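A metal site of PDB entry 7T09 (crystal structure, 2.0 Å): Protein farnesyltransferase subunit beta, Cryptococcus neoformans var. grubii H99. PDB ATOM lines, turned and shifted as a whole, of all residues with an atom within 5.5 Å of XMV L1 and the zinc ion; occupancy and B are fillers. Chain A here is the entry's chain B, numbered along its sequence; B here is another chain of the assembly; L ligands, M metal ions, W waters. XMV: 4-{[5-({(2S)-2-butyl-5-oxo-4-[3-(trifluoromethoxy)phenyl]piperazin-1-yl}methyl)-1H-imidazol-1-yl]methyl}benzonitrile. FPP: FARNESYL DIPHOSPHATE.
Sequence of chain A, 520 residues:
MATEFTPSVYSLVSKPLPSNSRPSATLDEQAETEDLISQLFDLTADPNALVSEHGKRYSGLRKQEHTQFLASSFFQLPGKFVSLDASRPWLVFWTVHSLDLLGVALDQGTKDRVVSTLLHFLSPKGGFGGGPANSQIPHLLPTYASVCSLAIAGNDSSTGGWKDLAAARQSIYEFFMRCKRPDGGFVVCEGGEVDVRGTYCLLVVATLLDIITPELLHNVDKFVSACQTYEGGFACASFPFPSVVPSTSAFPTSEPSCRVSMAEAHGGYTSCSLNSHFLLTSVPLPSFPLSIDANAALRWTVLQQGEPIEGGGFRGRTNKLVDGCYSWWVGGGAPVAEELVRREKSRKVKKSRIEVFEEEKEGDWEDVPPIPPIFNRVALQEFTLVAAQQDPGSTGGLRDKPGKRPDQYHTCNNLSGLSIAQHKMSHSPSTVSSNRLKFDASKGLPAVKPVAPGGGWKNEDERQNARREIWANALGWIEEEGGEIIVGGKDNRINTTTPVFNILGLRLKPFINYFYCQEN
N15 of XMV L1 is bound to the zinc ion, at 2.1 Å. NE2 of His 410 is bound to the zinc ion (2.1 Å). The zinc ion is bound by the side-chain carboxylate (OD1) of Asp 323 (2.2 Å). SG of Cys 325 is bound to the zinc ion (2.3 Å). OD2 of Asp 323 binds the zinc ion (2.5 Å).
Merely in contact with XMV L1: Leu 84 (3.9 Å), Ser 87 (3.5 Å), Trp 90 (3.1 Å), Trp 94 (3.3 Å), Tyr 326 (3.7 Å), Trp 329 (3.7 Å), Asp 407 (3.7 Å), Tyr 409 (3.3 Å) and Tyr 123 of chain B (3.6 Å). Hydrophobic or aromatic side chains that line XMV L1: Leu 84, Trp 90, Trp 94, Trp 329, Tyr 409, His 410 and Tyr 123 of chain B. The nearest printed residue that does not touch XMV L1 is Asn 413 (4.7 Å).
Merely in contact with the zinc ion: Tyr 409 (3.9 Å). Within 4 Å of the zinc ion: Asp 323, Cys 325, Tyr 409 and His 410.
The side-chain hydroxyl of Tyr 326 sits at hydrogen-bond distance from an oxygen (O3B) of FPP L2, at 2.6 Å. The guanidinium group of Arg 197 is in hydrogen-bond range of a nitrogen (N26) of XMV L1 (3.3 Å).
Water W3 bridges the indole nitrogen (NE1) of Trp 94 (2.9 Å) and the side-chain amide nitrogen (ND2) of Asn 413 (3.3 Å).
The side-chain carboxylate (OD1) of Asp 407 sits at hydrogen-bond distance from the backbone NH (N) of His 410 (2.7 Å). The side-chain hydroxyl of Tyr 409 sits at hydrogen-bond distance from the indole nitrogen of Trp 329 (3.0 Å). SG of Cys 325 sits close to OH of Tyr 409 (3.2 Å). The side-chain amide nitrogen of Asn 413 lies within hydrogen-bond range of the backbone carbonyl oxygen of Tyr 409. OD1 of Asp 407 is in hydrogen-bond range of N of Tyr 409 (2.9 Å).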
ATOM      1  N   LEU A  84      19.464 -19.998  37.969  1.00  0.00           N
ATOM      2  CA  LEU A  84      18.958 -19.917  36.596  1.00  0.00           C
ATOM      3  C   LEU A  84      17.521 -19.404  36.554  1.00  0.00           C
ATOM      4  O   LEU A  84      16.836 -19.553  35.530  1.00  0.00           O
ATOM      5  CB  LEU A  84      19.048 -21.274  35.915  1.00  0.00           C
ATOM      6  CG  LEU A  84      20.471 -21.781  35.636  1.00  0.00           C
ATOM      7  CD1 LEU A  84      20.497 -23.287  35.346  1.00  0.00           C
ATOM      8  CD2 LEU A  84      21.064 -21.000  34.481  1.00  0.00           C
ATOM      9  N   SER A  87      16.562 -17.482  33.660  1.00  0.00           N
ATOM     10  CA  SER A  87      16.827 -18.174  32.393  1.00  0.00           C
ATOM     11  C   SER A  87      15.902 -19.369  32.225  1.00  0.00           C
ATOM     12  O   SER A  87      16.257 -20.344  31.563  1.00  0.00           O
ATOM     13  CB  SER A  87      18.294 -18.612  32.311  1.00  0.00           C
ATOM     14  OG  SER A  87      19.170 -17.504  32.146  1.00  0.00           O
ATOM     15  N   TRP A  90      15.468 -21.008  28.891  1.00  0.00           N
ATOM     16  CA  TRP A  90      16.588 -21.845  28.480  1.00  0.00           C
ATOM     17  C   TRP A  90      16.438 -23.246  29.048  1.00  0.00           C
ATOM     18  O   TRP A  90      16.747 -24.238  28.364  1.00  0.00           O
ATOM     19  CB  TRP A  90      17.924 -21.234  28.930  1.00  0.00           C
ATOM     20  CG  TRP A  90      18.317 -20.017  28.136  1.00  0.00           C
ATOM     21  CD1 TRP A  90      18.249 -18.714  28.535  1.00  0.00           C
ATOM     22  CD2 TRP A  90      18.821 -19.994  26.781  1.00  0.00           C
ATOM     23  NE1 TRP A  90      18.699 -17.880  27.516  1.00  0.00           N
ATOM     24  CE2 TRP A  90      19.042 -18.648  26.440  1.00  0.00           C
ATOM     25  CE3 TRP A  90      19.107 -20.995  25.832  1.00  0.00           C
ATOM     26  CZ2 TRP A  90      19.540 -18.259  25.185  1.00  0.00           C
ATOM     27  CZ3 TRP A  90      19.605 -20.610  24.599  1.00  0.00           C
ATOM     28  CH2 TRP A  90      19.806 -19.258  24.282  1.00  0.00           C
ATOM     29  N   TRP A  94      16.586 -26.210  26.463  1.00  0.00           N
ATOM     30  CA  TRP A  94      17.551 -27.313  26.599  1.00  0.00           C
ATOM     31  C   TRP A  94      16.823 -28.641  26.709  1.00  0.00           C
ATOM     32  O   TRP A  94      17.276 -29.638  26.134  1.00  0.00           O
ATOM     33  CB  TRP A  94      18.464 -27.091  27.809  1.00  0.00           C
ATOM     34  CG  TRP A  94      19.390 -25.858  27.698  1.00  0.00           C
ATOM     35  CD1 TRP A  94      19.959 -25.346  26.569  1.00  0.00           C
ATOM     36  CD2 TRP A  94      19.818 -25.016  28.782  1.00  0.00           C
ATOM     37  NE1 TRP A  94      20.712 -24.232  26.876  1.00  0.00           N
ATOM     38  CE2 TRP A  94      20.643 -24.008  28.231  1.00  0.00           C
ATOM     39  CE3 TRP A  94      19.581 -25.017  30.165  1.00  0.00           C
ATOM     40  CZ2 TRP A  94      21.236 -23.006  29.013  1.00  0.00           C
ATOM     41  CZ3 TRP A  94      20.174 -24.014  30.946  1.00  0.00           C
ATOM     42  CH2 TRP A  94      20.993 -23.032  30.364  1.00  0.00           C
ATOM     43  N   LEU A 141      17.755 -12.863  24.992  1.00  0.00           N
ATOM     44  CA  LEU A 141      18.179 -14.258  24.993  1.00  0.00           C
ATOM     45  C   LEU A 141      17.010 -15.186  25.369  1.00  0.00           C
ATOM     46  O   LEU A 141      16.799 -16.192  24.671  1.00  0.00           O
ATOM     47  CB  LEU A 141      19.385 -14.479  25.915  1.00  0.00           C
ATOM     48  CG  LEU A 141      20.772 -14.316  25.288  1.00  0.00           C
ATOM     49  CD1 LEU A 141      20.929 -12.973  24.574  1.00  0.00           C
ATOM     50  CD2 LEU A 141      21.848 -14.481  26.364  1.00  0.00           C
ATOM     51  N   ARG A 197      25.877 -12.210  21.258  1.00  0.00           N
ATOM     52  CA  ARG A 197      24.767 -13.066  21.697  1.00  0.00           C
ATOM     53  C   ARG A 197      23.435 -12.377  21.446  1.00  0.00           C
ATOM     54  O   ARG A 197      22.466 -13.014  20.994  1.00  0.00           O
ATOM     55  CB  ARG A 197      24.881 -13.438  23.186  1.00  0.00           C
ATOM     56  CG  ARG A 197      26.150 -14.171  23.624  1.00  0.00           C
ATOM     57  CD  ARG A 197      26.225 -14.230  25.157  1.00  0.00           C
ATOM     58  NE  ARG A 197      26.046 -12.895  25.715  1.00  0.00           N
ATOM     59  CZ  ARG A 197      25.439 -12.619  26.867  1.00  0.00           C
ATOM     60  NH1 ARG A 197      24.953 -13.596  27.630  1.00  0.00           N
ATOM     61  NH2 ARG A 197      25.311 -11.351  27.255  1.00  0.00           N
ATOM     62  N   ASP A 323      35.775 -29.241  26.105  1.00  0.00           N
ATOM     63  CA  ASP A 323      34.516 -29.181  26.839  1.00  0.00           C
ATOM     64  C   ASP A 323      33.412 -29.582  25.864  1.00  0.00           C
ATOM     65  O   ASP A 323      33.314 -29.024  24.767  1.00  0.00           O
ATOM     66  CB  ASP A 323      34.303 -27.746  27.396  1.00  0.00           C
ATOM     67  CG  ASP A 323      32.950 -27.552  28.112  1.00  0.00           C
ATOM     68  OD1 ASP A 323      32.845 -26.588  28.915  1.00  0.00           O
ATOM     69  OD2 ASP A 323      31.993 -28.328  27.890  1.00  0.00           O
ATOM     70  N   GLY A 324      32.577 -30.539  26.287  1.00  0.00           N
ATOM     71  CA  GLY A 324      31.567 -31.075  25.389  1.00  0.00           C
ATOM     72  C   GLY A 324      30.609 -30.047  24.805  1.00  0.00           C
ATOM     73  O   GLY A 324      30.126 -30.231  23.685  1.00  0.00           O
ATOM     74  N   CYS A 325      30.324 -28.949  25.534  1.00  0.00           N
ATOM     75  CA  CYS A 325      29.339 -28.018  24.992  1.00  0.00           C
ATOM     76  C   CYS A 325      29.847 -27.320  23.722  1.00  0.00           C
ATOM     77  O   CYS A 325      29.035 -26.925  22.883  1.00  0.00           O
ATOM     78  CB  CYS A 325      28.889 -26.977  26.032  1.00  0.00           C
ATOM     79  SG  CYS A 325      30.193 -25.794  26.600  1.00  0.00           S
ATOM     80  N   TYR A 326      31.168 -27.203  23.555  1.00  0.00           N
ATOM     81  CA  TYR A 326      31.710 -26.613  22.331  1.00  0.00           C
ATOM     82  C   TYR A 326      31.592 -27.522  21.123  1.00  0.00           C
ATOM     83  O   TYR A 326      31.926 -27.093  20.020  1.00  0.00           O
ATOM     84  CB  TYR A 326      33.173 -26.206  22.564  1.00  0.00           C
ATOM     85  CG  TYR A 326      33.273 -25.202  23.679  1.00  0.00           C
ATOM     86  CD1 TYR A 326      32.488 -24.047  23.671  1.00  0.00           C
ATOM     87  CD2 TYR A 326      34.100 -25.420  24.776  1.00  0.00           C
ATOM     88  CE1 TYR A 326      32.548 -23.126  24.722  1.00  0.00           C
ATOM     89  CE2 TYR A 326      34.164 -24.502  25.835  1.00  0.00           C
ATOM     90  CZ  TYR A 326      33.386 -23.359  25.807  1.00  0.00           C
ATOM     91  OH  TYR A 326      33.463 -22.444  26.847  1.00  0.00           O
ATOM     92  N   TRP A 329      28.931 -25.235  19.840  1.00  0.00           N
ATOM     93  CA  TRP A 329      29.311 -23.840  19.576  1.00  0.00           C
ATOM     94  C   TRP A 329      30.424 -23.754  18.536  1.00  0.00           C
ATOM     95  O   TRP A 329      30.390 -22.878  17.662  1.00  0.00           O
ATOM     96  CB  TRP A 329      29.739 -23.126  20.865  1.00  0.00           C
ATOM     97  CG  TRP A 329      28.663 -23.106  21.911  1.00  0.00           C
ATOM     98  CD1 TRP A 329      28.733 -23.674  23.147  1.00  0.00           C
ATOM     99  CD2 TRP A 329      27.371 -22.501  21.818  1.00  0.00           C
ATOM    100  NE1 TRP A 329      27.557 -23.467  23.835  1.00  0.00           N
ATOM    101  CE2 TRP A 329      26.702 -22.756  23.032  1.00  0.00           C
ATOM    102  CE3 TRP A 329      26.705 -21.766  20.821  1.00  0.00           C
ATOM    103  CZ2 TRP A 329      25.403 -22.291  23.296  1.00  0.00           C
ATOM    104  CZ3 TRP A 329      25.396 -21.319  21.082  1.00  0.00           C
ATOM    105  CH2 TRP A 329      24.772 -21.577  22.309  1.00  0.00           C
ATOM    106  N   ASP A 400      30.353 -31.490  30.680  1.00  0.00           N
ATOM    107  CA  ASP A 400      31.531 -30.763  30.178  1.00  0.00           C
ATOM    108  C   ASP A 400      32.648 -31.783  29.903  1.00  0.00           C
ATOM    109  O   ASP A 400      33.036 -31.915  28.806  1.00  0.00           O
ATOM    110  CB  ASP A 400      31.925 -29.707  31.204  1.00  0.00           C
ATOM    111  CG  ASP A 400      33.341 -29.190  31.152  1.00  0.00           C
ATOM    112  OD1 ASP A 400      34.027 -29.520  30.259  1.00  0.00           O
ATOM    113  OD2 ASP A 400      33.667 -28.430  31.976  1.00  0.00           O
ATOM    114  N   ASP A 407      24.433 -31.531  33.299  1.00  0.00           N
ATOM    115  CA  ASP A 407      23.375 -30.544  33.451  1.00  0.00           C
ATOM    116  C   ASP A 407      22.622 -30.408  32.131  1.00  0.00           C
ATOM    117  O   ASP A 407      23.028 -30.940  31.092  1.00  0.00           O
ATOM    118  CB  ASP A 407      23.941 -29.199  33.943  1.00  0.00           C
ATOM    119  CG  ASP A 407      24.951 -28.610  32.975  1.00  0.00           C
ATOM    120  OD1 ASP A 407      24.607 -28.432  31.792  1.00  0.00           O
ATOM    121  OD2 ASP A 407      26.097 -28.293  33.386  1.00  0.00           O
ATOM    122  N   GLN A 408      21.482 -29.705  32.188  1.00  0.00           N
ATOM    123  CA  GLN A 408      20.649 -29.571  30.999  1.00  0.00           C
ATOM    124  C   GLN A 408      21.361 -28.836  29.865  1.00  0.00           C
ATOM    125  O   GLN A 408      21.170 -29.169  28.689  1.00  0.00           O
ATOM    126  CB  GLN A 408      19.330 -28.869  31.350  1.00  0.00           C
ATOM    127  CG  GLN A 408      18.423 -29.621  32.331  1.00  0.00           C
ATOM    128  CD  GLN A 408      18.805 -29.397  33.797  1.00  0.00           C
ATOM    129  OE1 GLN A 408      19.902 -28.910  34.115  1.00  0.00           O
ATOM    130  NE2 GLN A 408      17.891 -29.728  34.701  1.00  0.00           N
ATOM    131  N   TYR A 409      22.196 -27.840  30.202  1.00  0.00           N
ATOM    132  CA  TYR A 409      22.891 -27.069  29.173  1.00  0.00           C
ATOM    133  C   TYR A 409      23.918 -27.910  28.424  1.00  0.00           C
ATOM    134  O   TYR A 409      24.005 -27.844  27.197  1.00  0.00           O
ATOM    135  CB  TYR A 409      23.545 -25.820  29.807  1.00  0.00           C
ATOM    136  CG  TYR A 409      24.687 -25.228  29.004  1.00  0.00           C
ATOM    137  CD1 TYR A 409      24.448 -24.246  28.035  1.00  0.00           C
ATOM    138  CD2 TYR A 409      25.998 -25.632  29.210  1.00  0.00           C
ATOM    139  CE1 TYR A 409      25.501 -23.695  27.279  1.00  0.00           C
ATOM    140  CE2 TYR A 409      27.061 -25.067  28.479  1.00  0.00           C
ATOM    141  CZ  TYR A 409      26.799 -24.121  27.516  1.00  0.00           C
ATOM    142  OH  TYR A 409      27.850 -23.606  26.781  1.00  0.00           O
ATOM    143  N   HIS A 410      24.704 -28.719  29.146  1.00  0.00           N
ATOM    144  CA  HIS A 410      25.640 -29.590  28.451  1.00  0.00           C
ATOM    145  C   HIS A 410      24.926 -30.746  27.742  1.00  0.00           C
ATOM    146  O   HIS A 410      25.446 -31.283  26.766  1.00  0.00           O
ATOM    147  CB  HIS A 410      26.719 -30.105  29.411  1.00  0.00           C
ATOM    148  CG  HIS A 410      27.733 -29.063  29.780  1.00  0.00           C
ATOM    149  ND1 HIS A 410      27.708 -28.386  30.978  1.00  0.00           N
ATOM    150  CD2 HIS A 410      28.768 -28.546  29.077  1.00  0.00           C
ATOM    151  CE1 HIS A 410      28.699 -27.514  31.013  1.00  0.00           C
ATOM    152  NE2 HIS A 410      29.362 -27.592  29.873  1.00  0.00           N
ATOM    153  N   ASN A 413      23.782 -29.140  24.338  1.00  0.00           N
ATOM    154  CA  ASN A 413      24.829 -28.727  23.408  1.00  0.00           C
ATOM    155  C   ASN A 413      25.747 -29.874  23.027  1.00  0.00           C
ATOM    156  O   ASN A 413      26.219 -29.917  21.883  1.00  0.00           O
ATOM    157  CB  ASN A 413      25.601 -27.546  23.994  1.00  0.00           C
ATOM    158  CG  ASN A 413      24.805 -26.246  23.912  1.00  0.00           C
ATOM    159  OD1 ASN A 413      24.539 -25.748  22.830  1.00  0.00           O
ATOM    160  ND2 ASN A 413      24.397 -25.708  25.061  1.00  0.00           N
ATOM    161  N   TYR B 123      27.391 -12.047  34.160  1.00  0.00           N
ATOM    162  CA  TYR B 123      27.379 -10.928  33.215  1.00  0.00           C
ATOM    163  C   TYR B 123      26.785  -9.681  33.855  1.00  0.00           C
ATOM    164  O   TYR B 123      27.231  -8.562  33.585  1.00  0.00           O
ATOM    165  CB  TYR B 123      26.535 -11.275  31.978  1.00  0.00           C
ATOM    166  CG  TYR B 123      27.147 -12.116  30.878  1.00  0.00           C
ATOM    167  CD1 TYR B 123      27.832 -11.539  29.806  1.00  0.00           C
ATOM    168  CD2 TYR B 123      26.974 -13.507  30.871  1.00  0.00           C
ATOM    169  CE1 TYR B 123      28.366 -12.337  28.772  1.00  0.00           C
ATOM    170  CE2 TYR B 123      27.487 -14.307  29.845  1.00  0.00           C
ATOM    171  CZ  TYR B 123      28.181 -13.716  28.799  1.00  0.00           C
ATOM    172  OH  TYR B 123      28.683 -14.514  27.791  1.00  0.00           O
HETATM  173  C10 XMV L   1      27.660 -20.312  32.383  1.00  0.00           C
HETATM  174  C13 XMV L   1      29.807 -22.854  31.090  1.00  0.00           C
HETATM  175  C20 XMV L   1      28.794 -20.623  28.436  1.00  0.00           C
HETATM  176  C21 XMV L   1      27.784 -19.766  28.003  1.00  0.00           C
HETATM  177  C22 XMV L   1      27.734 -18.448  28.458  1.00  0.00           C
HETATM  178  C24 XMV L   1      29.718 -18.827  29.770  1.00  0.00           C
HETATM  179  C28 XMV L   1      23.994 -19.876  29.083  1.00  0.00           C
HETATM  180  C01 XMV L   1      23.444 -25.365  33.790  1.00  0.00           C
HETATM  181  C02 XMV L   1      24.498 -24.276  34.031  1.00  0.00           C
HETATM  182  C03 XMV L   1      25.321 -23.983  32.775  1.00  0.00           C
HETATM  183  C04 XMV L   1      26.296 -22.791  32.942  1.00  0.00           C
HETATM  184  C05 XMV L   1      26.970 -22.379  31.533  1.00  0.00           C
HETATM  185  C06 XMV L   1      25.916 -21.820  30.640  1.00  0.00           C
HETATM  186  C08 XMV L   1      26.298 -19.675  31.864  1.00  0.00           C
HETATM  187  C12 XMV L   1      29.122 -22.007  32.191  1.00  0.00           C
HETATM  188  C14 XMV L   1      29.720 -24.229  30.991  1.00  0.00           C
HETATM  189  C16 XMV L   1      30.941 -23.484  29.344  1.00  0.00           C
HETATM  190  C18 XMV L   1      30.936 -21.030  29.816  1.00  0.00           C
HETATM  191  C19 XMV L   1      29.768 -20.144  29.314  1.00  0.00           C
HETATM  192  C23 XMV L   1      28.695 -17.975  29.341  1.00  0.00           C
HETATM  193  C25 XMV L   1      26.616 -17.504  27.995  1.00  0.00           C
HETATM  194  C27 XMV L   1      24.184 -19.979  30.450  1.00  0.00           C
HETATM  195  C29 XMV L   1      22.805 -19.398  28.546  1.00  0.00           C
HETATM  196  C30 XMV L   1      21.803 -19.008  29.421  1.00  0.00           C
HETATM  197  C31 XMV L   1      21.982 -19.096  30.800  1.00  0.00           C
HETATM  198  C32 XMV L   1      23.178 -19.585  31.317  1.00  0.00           C
HETATM  199  C34 XMV L   1      23.269 -20.186  26.297  1.00  0.00           C
HETATM  200  F35 XMV L   1      23.124 -21.466  26.749  1.00  0.00           F
HETATM  201  F36 XMV L   1      24.595 -19.899  26.200  1.00  0.00           F
HETATM  202  F37 XMV L   1      22.728 -20.086  25.053  1.00  0.00           F
HETATM  203  N07 XMV L   1      25.448 -20.495  30.972  1.00  0.00           N
HETATM  204  N11 XMV L   1      28.031 -21.467  31.707  1.00  0.00           N
HETATM  205  N15 XMV L   1      30.420 -24.594  29.924  1.00  0.00           N
HETATM  206  N17 XMV L   1      30.555 -22.425  30.080  1.00  0.00           N
HETATM  207  N26 XMV L   1      25.788 -16.808  27.657  1.00  0.00           N
HETATM  208  O09 XMV L   1      25.966 -18.571  32.181  1.00  0.00           O
HETATM  209  O33 XMV L   1      22.615 -19.278  27.150  1.00  0.00           O
HETATM  210  C1  FPP L   2      33.858 -18.086  28.870  1.00  0.00           C
HETATM  211  O1  FPP L   2      33.487 -18.846  30.002  1.00  0.00           O
HETATM  212  C2  FPP L   2      32.697 -17.965  27.849  1.00  0.00           C
HETATM  213  C3  FPP L   2      31.948 -16.858  27.674  1.00  0.00           C
HETATM  214  C4  FPP L   2      32.196 -15.581  28.484  1.00  0.00           C
HETATM  215  C5  FPP L   2      30.810 -16.825  26.630  1.00  0.00           C
HETATM  216  C6  FPP L   2      30.511 -18.195  25.981  1.00  0.00           C
HETATM  217  C7  FPP L   2      29.192 -18.128  25.163  1.00  0.00           C
HETATM  218  C8  FPP L   2      28.591 -19.230  24.710  1.00  0.00           C
HETATM  219  C10 FPP L   2      29.205 -20.623  24.965  1.00  0.00           C
HETATM  220  C9  FPP L   2      27.293 -19.221  23.905  1.00  0.00           C
HETATM  221  C11 FPP L   2      26.552 -17.887  23.787  1.00  0.00           C
HETATM  222  C12 FPP L   2      25.391 -18.057  22.784  1.00  0.00           C
HETATM  223  C13 FPP L   2      24.129 -17.696  22.999  1.00  0.00           C
HETATM  224  C14 FPP L   2      23.649 -17.033  24.305  1.00  0.00           C
HETATM  225  C15 FPP L   2      23.106 -17.932  21.880  1.00  0.00           C
HETATM  226  PA  FPP L   2      34.538 -19.858  30.799  1.00  0.00           P
HETATM  227  O1A FPP L   2      33.827 -20.292  32.049  1.00  0.00           O
HETATM  228  O2A FPP L   2      35.847 -19.146  31.080  1.00  0.00           O
HETATM  229  O3A FPP L   2      34.830 -21.183  29.898  1.00  0.00           O
HETATM  230  PB  FPP L   2      36.115 -21.493  28.939  1.00  0.00           P
HETATM  231  O1B FPP L   2      37.258 -21.851  29.855  1.00  0.00           O
HETATM  232  O2B FPP L   2      36.450 -20.332  28.054  1.00  0.00           O
HETATM  233  O3B FPP L   2      35.696 -22.693  28.088  1.00  0.00           O
HETATM  234 ZN    ZN M   1      30.695 -26.353  28.798  1.00  0.00          ZN
HETATM  235  O   HOH W   1      27.946 -16.742  33.269  1.00  0.00           O
HETATM  236  O   HOH W   2      33.421 -23.213  31.838  1.00  0.00           O
HETATM  237  O   HOH W   3      22.159 -23.355  24.568  1.00  0.00           O
